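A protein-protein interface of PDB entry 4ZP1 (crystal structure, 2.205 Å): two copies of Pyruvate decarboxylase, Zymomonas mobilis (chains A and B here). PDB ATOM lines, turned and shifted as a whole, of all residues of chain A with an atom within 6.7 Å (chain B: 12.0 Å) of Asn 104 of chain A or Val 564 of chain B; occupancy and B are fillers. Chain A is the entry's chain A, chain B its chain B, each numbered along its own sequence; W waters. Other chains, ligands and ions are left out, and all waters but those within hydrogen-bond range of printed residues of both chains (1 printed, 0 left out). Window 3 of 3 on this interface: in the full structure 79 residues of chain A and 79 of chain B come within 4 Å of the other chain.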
ATOM      1  N   PRO A 101     -33.591   1.074 -14.431  1.00  0.00           N
ATOM      2  CA  PRO A 101     -32.422   1.417 -15.246  1.00  0.00           C
ATOM      3  C   PRO A 101     -31.740   0.200 -15.863  1.00  0.00           C
ATOM      4  O   PRO A 101     -31.870  -0.930 -15.372  1.00  0.00           O
ATOM      5  CB  PRO A 101     -31.495   2.105 -14.241  1.00  0.00           C
ATOM      6  CG  PRO A 101     -32.431   2.721 -13.250  1.00  0.00           C
ATOM      7  CD  PRO A 101     -33.554   1.732 -13.111  1.00  0.00           C
ATOM      8  N   ASN A 102     -31.039   0.453 -16.960  1.00  0.00           N
ATOM      9  CA  ASN A 102     -30.130  -0.508 -17.560  1.00  0.00           C
ATOM     10  C   ASN A 102     -29.152  -1.049 -16.518  1.00  0.00           C
ATOM     11  O   ASN A 102     -28.537  -0.275 -15.784  1.00  0.00           O
ATOM     12  CB  ASN A 102     -29.369   0.152 -18.714  1.00  0.00           C
ATOM     13  CG  ASN A 102     -28.703  -0.857 -19.625  1.00  0.00           C
ATOM     14  OD1 ASN A 102     -27.716  -1.494 -19.250  1.00  0.00           O
ATOM     15  ND2 ASN A 102     -29.238  -1.005 -20.834  1.00  0.00           N
ATOM     16  N   ASN A 103     -28.991  -2.366 -16.458  1.00  0.00           N
ATOM     17  CA  ASN A 103     -28.207  -2.967 -15.380  1.00  0.00           C
ATOM     18  C   ASN A 103     -26.716  -2.697 -15.537  1.00  0.00           C
ATOM     19  O   ASN A 103     -25.949  -2.847 -14.587  1.00  0.00           O
ATOM     20  CB  ASN A 103     -28.485  -4.482 -15.275  1.00  0.00           C
ATOM     21  CG  ASN A 103     -27.858  -5.291 -16.407  1.00  0.00           C
ATOM     22  OD1 ASN A 103     -27.662  -4.797 -17.521  1.00  0.00           O
ATOM     23  ND2 ASN A 103     -27.553  -6.554 -16.122  1.00  0.00           N
ATOM     24  N   ASN A 104     -26.306  -2.288 -16.735  1.00  0.00           N
ATOM     25  CA  ASN A 104     -24.955  -1.783 -16.944  1.00  0.00           C
ATOM     26  C   ASN A 104     -24.704  -0.467 -16.199  1.00  0.00           C
ATOM     27  O   ASN A 104     -23.560  -0.135 -15.871  1.00  0.00           O
ATOM     28  CB  ASN A 104     -24.684  -1.591 -18.437  1.00  0.00           C
ATOM     29  CG  ASN A 104     -24.555  -2.908 -19.177  1.00  0.00           C
ATOM     30  OD1 ASN A 104     -23.710  -3.740 -18.844  1.00  0.00           O
ATOM     31  ND2 ASN A 104     -25.407  -3.113 -20.175  1.00  0.00           N
ATOM     32  N   ASP A 105     -25.771   0.278 -15.930  1.00  0.00           N
ATOM     33  CA  ASP A 105     -25.638   1.569 -15.254  1.00  0.00           C
ATOM     34  C   ASP A 105     -25.513   1.433 -13.741  1.00  0.00           C
ATOM     35  O   ASP A 105     -25.452   2.431 -13.034  1.00  0.00           O
ATOM     36  CB  ASP A 105     -26.823   2.466 -15.592  1.00  0.00           C
ATOM     37  CG  ASP A 105     -26.856   2.852 -17.058  1.00  0.00           C
ATOM     38  OD1 ASP A 105     -25.773   3.101 -17.639  1.00  0.00           O
ATOM     39  OD2 ASP A 105     -27.968   2.906 -17.626  1.00  0.00           O
ATOM     40  N   HIS A 106     -25.467   0.195 -13.255  1.00  0.00           N
ATOM     41  CA  HIS A 106     -25.314  -0.076 -11.832  1.00  0.00           C
ATOM     42  C   HIS A 106     -23.843  -0.093 -11.416  1.00  0.00           C
ATOM     43  O   HIS A 106     -22.985  -0.586 -12.158  1.00  0.00           O
ATOM     44  CB  HIS A 106     -25.974  -1.409 -11.485  1.00  0.00           C
ATOM     45  CG  HIS A 106     -26.659  -1.419 -10.159  1.00  0.00           C
ATOM     46  ND1 HIS A 106     -27.874  -2.036  -9.955  1.00  0.00           N
ATOM     47  CD2 HIS A 106     -26.301  -0.889  -8.966  1.00  0.00           C
ATOM     48  CE1 HIS A 106     -28.236  -1.883  -8.695  1.00  0.00           C
ATOM     49  NE2 HIS A 106     -27.297  -1.194  -8.071  1.00  0.00           N
ATOM     50  N   ALA A 107     -23.563   0.441 -10.227  1.00  0.00           N
ATOM     51  CA  ALA A 107     -22.203   0.510  -9.675  1.00  0.00           C
ATOM     52  C   ALA A 107     -21.183   1.017 -10.695  1.00  0.00           C
ATOM     53  O   ALA A 107     -20.018   0.615 -10.675  1.00  0.00           O
ATOM     54  CB  ALA A 107     -21.775  -0.857  -9.144  1.00  0.00           C
ATOM     55  N   ALA A 108     -21.632   1.897 -11.585  1.00  0.00           N
ATOM     56  CA  ALA A 108     -20.786   2.432 -12.643  1.00  0.00           C
ATOM     57  C   ALA A 108     -20.445   3.886 -12.368  1.00  0.00           C
ATOM     58  O   ALA A 108     -19.484   4.424 -12.916  1.00  0.00           O
ATOM     59  CB  ALA A 108     -21.473   2.296 -13.989  1.00  0.00           C
ATOM     60  N   HIS A 110     -23.025   6.235 -12.689  1.00  0.00           N
ATOM     61  CA  HIS A 110     -23.799   6.848 -13.763  1.00  0.00           C
ATOM     62  C   HIS A 110     -25.003   7.623 -13.249  1.00  0.00           C
ATOM     63  O   HIS A 110     -25.914   7.062 -12.632  1.00  0.00           O
ATOM     64  CB  HIS A 110     -24.275   5.792 -14.766  1.00  0.00           C
ATOM     65  CG  HIS A 110     -23.234   5.376 -15.759  1.00  0.00           C
ATOM     66  ND1 HIS A 110     -23.547   4.751 -16.946  1.00  0.00           N
ATOM     67  CD2 HIS A 110     -21.884   5.486 -15.738  1.00  0.00           C
ATOM     68  CE1 HIS A 110     -22.437   4.495 -17.615  1.00  0.00           C
ATOM     69  NE2 HIS A 110     -21.414   4.929 -16.903  1.00  0.00           N
ATOM     70  N   ASN A 169     -33.238  -3.540 -19.900  1.00  0.00           N
ATOM     71  CA  ASN A 169     -32.535  -4.287 -20.937  1.00  0.00           C
ATOM     72  C   ASN A 169     -32.555  -5.803 -20.742  1.00  0.00           C
ATOM     73  O   ASN A 169     -31.823  -6.523 -21.420  1.00  0.00           O
ATOM     74  CB  ASN A 169     -31.085  -3.810 -21.032  1.00  0.00           C
ATOM     75  CG  ASN A 169     -30.294  -4.108 -19.777  1.00  0.00           C
ATOM     76  OD1 ASN A 169     -30.833  -4.088 -18.671  1.00  0.00           O
ATOM     77  ND2 ASN A 169     -29.007  -4.390 -19.941  1.00  0.00           N
ATOM     78  N   ASP B 289     -27.352  10.512 -18.959  1.00  0.00           N
ATOM     79  CA  ASP B 289     -27.492   9.820 -20.236  1.00  0.00           C
ATOM     80  C   ASP B 289     -28.156  10.698 -21.297  1.00  0.00           C
ATOM     81  O   ASP B 289     -27.852  10.580 -22.482  1.00  0.00           O
ATOM     82  CB  ASP B 289     -28.279   8.514 -20.056  1.00  0.00           C
ATOM     83  CG  ASP B 289     -29.615   8.723 -19.376  1.00  0.00           C
ATOM     84  OD1 ASP B 289     -29.671   9.505 -18.408  1.00  0.00           O
ATOM     85  OD2 ASP B 289     -30.610   8.106 -19.813  1.00  0.00           O
ATOM     86  N   GLY B 294     -26.740   9.937 -24.856  1.00  0.00           N
ATOM     87  CA  GLY B 294     -26.526   8.500 -24.842  1.00  0.00           C
ATOM     88  C   GLY B 294     -25.078   8.094 -24.638  1.00  0.00           C
ATOM     89  O   GLY B 294     -24.627   7.089 -25.185  1.00  0.00           O
ATOM     90  N   TRP B 295     -24.352   8.873 -23.841  1.00  0.00           N
ATOM     91  CA  TRP B 295     -22.947   8.601 -23.539  1.00  0.00           C
ATOM     92  C   TRP B 295     -22.068   8.684 -24.783  1.00  0.00           C
ATOM     93  O   TRP B 295     -20.965   8.145 -24.804  1.00  0.00           O
ATOM     94  CB  TRP B 295     -22.789   7.225 -22.878  1.00  0.00           C
ATOM     95  CG  TRP B 295     -23.734   6.996 -21.743  1.00  0.00           C
ATOM     96  CD1 TRP B 295     -24.718   6.057 -21.678  1.00  0.00           C
ATOM     97  CD2 TRP B 295     -23.807   7.738 -20.516  1.00  0.00           C
ATOM     98  NE1 TRP B 295     -25.391   6.156 -20.485  1.00  0.00           N
ATOM     99  CE2 TRP B 295     -24.853   7.183 -19.754  1.00  0.00           C
ATOM    100  CE3 TRP B 295     -23.086   8.813 -19.986  1.00  0.00           C
ATOM    101  CZ2 TRP B 295     -25.199   7.668 -18.489  1.00  0.00           C
ATOM    102  CZ3 TRP B 295     -23.427   9.289 -18.733  1.00  0.00           C
ATOM    103  CH2 TRP B 295     -24.472   8.714 -17.997  1.00  0.00           C
ATOM    104  N   ILE B 298     -19.253  12.788 -24.311  1.00  0.00           N
ATOM    105  CA  ILE B 298     -18.729  12.990 -22.967  1.00  0.00           C
ATOM    106  C   ILE B 298     -17.492  13.866 -23.050  1.00  0.00           C
ATOM    107  O   ILE B 298     -16.685  13.710 -23.962  1.00  0.00           O
ATOM    108  CB  ILE B 298     -18.377  11.652 -22.279  1.00  0.00           C
ATOM    109  CG1 ILE B 298     -19.582  10.709 -22.282  1.00  0.00           C
ATOM    110  CG2 ILE B 298     -17.883  11.896 -20.860  1.00  0.00           C
ATOM    111  CD1 ILE B 298     -19.295   9.333 -21.698  1.00  0.00           C
ATOM    112  N   VAL B 555     -30.468   7.761 -27.505  1.00  0.00           N
ATOM    113  CA  VAL B 555     -31.030   7.493 -26.191  1.00  0.00           C
ATOM    114  C   VAL B 555     -31.604   6.089 -26.138  1.00  0.00           C
ATOM    115  O   VAL B 555     -31.408   5.364 -25.164  1.00  0.00           O
ATOM    116  CB  VAL B 555     -32.126   8.508 -25.831  1.00  0.00           C
ATOM    117  CG1 VAL B 555     -32.988   7.980 -24.693  1.00  0.00           C
ATOM    118  CG2 VAL B 555     -31.503   9.859 -25.482  1.00  0.00           C
ATOM    119  N   ALA B 556     -32.312   5.705 -27.195  1.00  0.00           N
ATOM    120  CA  ALA B 556     -32.888   4.376 -27.265  1.00  0.00           C
ATOM    121  C   ALA B 556     -31.775   3.332 -27.266  1.00  0.00           C
ATOM    122  O   ALA B 556     -31.898   2.283 -26.630  1.00  0.00           O
ATOM    123  CB  ALA B 556     -33.759   4.236 -28.499  1.00  0.00           C
ATOM    124  N   ALA B 557     -30.681   3.638 -27.963  1.00  0.00           N
ATOM    125  CA  ALA B 557     -29.550   2.715 -28.054  1.00  0.00           C
ATOM    126  C   ALA B 557     -28.887   2.520 -26.693  1.00  0.00           C
ATOM    127  O   ALA B 557     -28.581   1.391 -26.298  1.00  0.00           O
ATOM    128  CB  ALA B 557     -28.537   3.213 -29.073  1.00  0.00           C
ATOM    129  N   ALA B 558     -28.667   3.624 -25.982  1.00  0.00           N
ATOM    130  CA  ALA B 558     -28.068   3.572 -24.651  1.00  0.00           C
ATOM    131  C   ALA B 558     -28.906   2.734 -23.679  1.00  0.00           C
ATOM    132  O   ALA B 558     -28.372   1.889 -22.957  1.00  0.00           O
ATOM    133  CB  ALA B 558     -27.880   4.977 -24.104  1.00  0.00           C
ATOM    134  N   ASN B 559     -30.215   2.973 -23.671  1.00  0.00           N
ATOM    135  CA  ASN B 559     -31.123   2.279 -22.759  1.00  0.00           C
ATOM    136  C   ASN B 559     -31.217   0.785 -23.028  1.00  0.00           C
ATOM    137  O   ASN B 559     -31.451  -0.006 -22.117  1.00  0.00           O
ATOM    138  CB  ASN B 559     -32.522   2.894 -22.835  1.00  0.00           C
ATOM    139  CG  ASN B 559     -32.599   4.255 -22.171  1.00  0.00           C
ATOM    140  OD1 ASN B 559     -31.575   4.869 -21.862  1.00  0.00           O
ATOM    141  ND2 ASN B 559     -33.818   4.737 -21.949  1.00  0.00           N
ATOM    142  N   SER B 560     -31.023   0.401 -24.285  1.00  0.00           N
ATOM    143  CA  SER B 560     -31.242  -0.978 -24.702  1.00  0.00           C
ATOM    144  C   SER B 560     -29.990  -1.851 -24.680  1.00  0.00           C
ATOM    145  O   SER B 560     -30.089  -3.062 -24.851  1.00  0.00           O
ATOM    146  CB  SER B 560     -31.843  -1.006 -26.112  1.00  0.00           C
ATOM    147  OG  SER B 560     -33.129  -0.414 -26.135  1.00  0.00           O
ATOM    148  N   ARG B 561     -28.818  -1.253 -24.479  1.00  0.00           N
ATOM    149  CA  ARG B 561     -27.570  -2.005 -24.613  1.00  0.00           C
ATOM    150  C   ARG B 561     -27.538  -3.186 -23.647  1.00  0.00           C
ATOM    151  O   ARG B 561     -27.867  -3.056 -22.468  1.00  0.00           O
ATOM    152  CB  ARG B 561     -26.348  -1.097 -24.412  1.00  0.00           C
ATOM    153  CG  ARG B 561     -26.091  -0.606 -22.989  1.00  0.00           C
ATOM    154  CD  ARG B 561     -25.149   0.618 -22.994  1.00  0.00           C
ATOM    155  NE  ARG B 561     -24.501   0.829 -21.697  1.00  0.00           N
ATOM    156  CZ  ARG B 561     -25.016   1.555 -20.707  1.00  0.00           C
ATOM    157  NH1 ARG B 561     -26.190   2.148 -20.862  1.00  0.00           N
ATOM    158  NH2 ARG B 561     -24.357   1.685 -19.562  1.00  0.00           N
ATOM    159  N   LYS B 562     -27.168  -4.349 -24.170  1.00  0.00           N
ATOM    160  CA  LYS B 562     -27.166  -5.570 -23.377  1.00  0.00           C
ATOM    161  C   LYS B 562     -26.093  -5.513 -22.292  1.00  0.00           C
ATOM    162  O   LYS B 562     -25.198  -4.664 -22.346  1.00  0.00           O
ATOM    163  CB  LYS B 562     -26.960  -6.785 -24.281  1.00  0.00           C
ATOM    164  CG  LYS B 562     -25.746  -6.687 -25.172  1.00  0.00           C
ATOM    165  CD  LYS B 562     -25.734  -7.811 -26.187  1.00  0.00           C
ATOM    166  CE  LYS B 562     -26.969  -7.748 -27.069  1.00  0.00           C
ATOM    167  NZ  LYS B 562     -26.952  -8.799 -28.122  1.00  0.00           N
ATOM    168  N   PRO B 563     -26.193  -6.412 -21.296  1.00  0.00           N
ATOM    169  CA  PRO B 563     -25.272  -6.485 -20.151  1.00  0.00           C
ATOM    170  C   PRO B 563     -23.866  -6.975 -20.515  1.00  0.00           C
ATOM    171  O   PRO B 563     -23.670  -7.591 -21.566  1.00  0.00           O
ATOM    172  CB  PRO B 563     -25.957  -7.493 -19.211  1.00  0.00           C
ATOM    173  CG  PRO B 563     -27.365  -7.627 -19.709  1.00  0.00           C
ATOM    174  CD  PRO B 563     -27.291  -7.388 -21.179  1.00  0.00           C
ATOM    175  N   VAL B 564     -22.907  -6.706 -19.632  1.00  0.00           N
ATOM    176  CA  VAL B 564     -21.539  -7.197 -19.788  1.00  0.00           C
ATOM    177  C   VAL B 564     -21.174  -8.148 -18.648  1.00  0.00           C
ATOM    178  O   VAL B 564     -21.526  -7.900 -17.493  1.00  0.00           O
ATOM    179  CB  VAL B 564     -20.517  -6.043 -19.819  1.00  0.00           C
ATOM    180  CG1 VAL B 564     -19.100  -6.596 -19.906  1.00  0.00           C
ATOM    181  CG2 VAL B 564     -20.808  -5.094 -20.978  1.00  0.00           C
ATOM    182  N   ASN B 565     -20.470  -9.232 -18.975  1.00  0.00           N
ATOM    183  CA  ASN B 565     -20.039 -10.208 -17.974  1.00  0.00           C
ATOM    184  C   ASN B 565     -19.145  -9.594 -16.899  1.00  0.00           C
ATOM    185  O   ASN B 565     -18.276  -8.773 -17.198  1.00  0.00           O
ATOM    186  CB  ASN B 565     -19.305 -11.372 -18.647  1.00  0.00           C
ATOM    187  CG  ASN B 565     -18.783 -12.392 -17.646  1.00  0.00           C
ATOM    188  OD1 ASN B 565     -17.638 -12.313 -17.196  1.00  0.00           O
ATOM    189  ND2 ASN B 565     -19.624 -13.358 -17.295  1.00  0.00           N
ATOM    190  N   LYS B 566     -19.362 -10.000 -15.650  1.00  0.00           N
ATOM    191  CA  LYS B 566     -18.583  -9.483 -14.526  1.00  0.00           C
ATOM    192  C   LYS B 566     -18.410 -10.530 -13.428  1.00  0.00           C
ATOM    193  O   LYS B 566     -17.301 -10.759 -12.942  1.00  0.00           O
ATOM    194  CB  LYS B 566     -19.242  -8.221 -13.957  1.00  0.00           C
ATOM    195  CG  LYS B 566     -20.721  -8.377 -13.627  1.00  0.00           C
ATOM    196  CD  LYS B 566     -21.328  -7.052 -13.171  1.00  0.00           C
ATOM    197  CE  LYS B 566     -22.797  -7.208 -12.795  1.00  0.00           C
ATOM    198  NZ  LYS B 566     -23.374  -5.965 -12.224  1.00  0.00           N
HETATM  199  O   HOH W   1     -27.863   4.512 -20.103  1.00  0.00           O
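Of chain B, only Pro 563 comes within 4 Å of Asn 103 of chain A.
Asn 104 of chain A touches just these residues of chain B: Arg 561, Lys 562, Pro 563 and Val 564.
Of chain B, only Arg 561 comes within 4 Å of Asp 105 of chain A.
No residue of chain B comes within 4 Å of Ala 107 of chain A.
No residue of chain B comes within 4 Å of Ala 108 of chain A.
Printed residues of chain B within 4 Å of His 110 of chain A: Trp 295 (3.7 Å) and Arg 561 (3.9 Å).
Of the printed residues of chain A, Trp 295 of chain B touches His 110 (3.7 Å).
Of chain A, only Asn 104 (3.2 Å) comes within 4 Å of Val 564 of chain B.
The nearest residue of chain A that does not touch Val 564 of chain B is Asn 103 of chain A (5.5 Å).
The nearest printed residue of chain B that does not touch Asn 169 of chain A is Ser 560 of chain B (4.02 Å).
Asn 102 of chain A touches Ala 558 of chain B (ND2 to O, 3.7 Å).
Pro 563 of chain B touches Asn 103 of chain A.
Pro 563 of chain B touches Asn 104 of chain A (CA to ND2, 3.4 Å).
His 110 of chain A touches Trp 295 of chain B.
NH2 of Arg 561 of chain B touches CE1 of His 110 of chain A (3.9 Å).
CB of Asn 169 of chain A touches O of Asn 559 of chain B, 3.97 Å away.
Asn 169 of chain A touches Lys 562 of chain B (ND2 to C, 3.9 Å).
ND2 of Asn 169 of chain A touches CG of Pro 563 of chain B, at 3.6 Å.
OD1 of Asp 105 of chain A sits at hydrogen-bond distance from ND1 of His 110 of chain A.
O of Ala 558 of chain B is in hydrogen-bond range of NH1 of Arg 561 of chain B, at 3.0 Å.
The side-chain amide oxygen (OD1) of Asn 102 of chain A lies within hydrogen-bond range of the side-chain amide nitrogen (ND2) of Asn 169 of chain A, at 3.2 Å.
The side-chain amide oxygen (OD1) of Asn 102 of chain A sits at hydrogen-bond distance from the side-chain amide nitrogen (ND2) of Asn 104 of chain A, 3.0 Å away.
The side-chain amide oxygen (OD1) of Asn 559 of chain B lies close to the backbone carbonyl oxygen (O) of Val 555 of chain B, 3.3 Å away.
OD1 of Asn 103 of chain A is in hydrogen-bond range of ND2 of Asn 169 of chain A, 2.8 Å away.
Water W1 lies within hydrogen-bond range of the side-chain carboxylate (OD2) of Asp 105 of chain A, the indole nitrogen (NE1) of Trp 295 of chain B and the guanidinium group (NH1) of Arg 561 of chain B.
The side-chain carboxylate (OD1) of Asp 105 of chain A lies within salt-bridge range of the guanidinium group (NH2) of Arg 561 of chain B.
The side-chain amide nitrogen of Asn 102 of chain A lies within hydrogen-bond range of the backbone carbonyl oxygen of Asn 559 of chain B.
The side-chain amide oxygen (OD1) of Asn 104 of chain A lies within hydrogen-bond range of the backbone NH (N) of Val 564 of chain B (3.2 Å).
O of Lys 562 of chain B is in hydrogen-bond range of ND2 of Asn 104 of chain A, 2.7 Å away.
The backbone carbonyl oxygen of Arg 561 of chain B sits at hydrogen-bond distance from the side-chain amide nitrogen of Asn 169 of chain A, at 3.1 Å.
The backbone carbonyl oxygen (O) of Arg 561 of chain B is in hydrogen-bond range of the side-chain amide nitrogen (ND2) of Asn 102 of chain A, 3.0 Å away.
The backbone carbonyl oxygen of Arg 561 of chain B is in hydrogen-bond range of the side-chain amide nitrogen of Asn 104 of chain A, 3.4 Å away.
No position is printed for both chains.
Printed residues of chain B that touch a printed residue of chain A: Trp 295, Ala 558, Asn 559, Arg 561, Lys 562, Pro 563 and Val 564.
Hydrophobic or aromatic side chains of chain A that line the printed part of chain B: His 110.
Among the printed residues, 15 pairs touch across the chains.
Among the printed residues, Asp or Glu carboxylates within 4 Å of a Lys or Arg side-chain nitrogen of the other chain: Asp 105 of chain A with Arg 561 of chain B.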
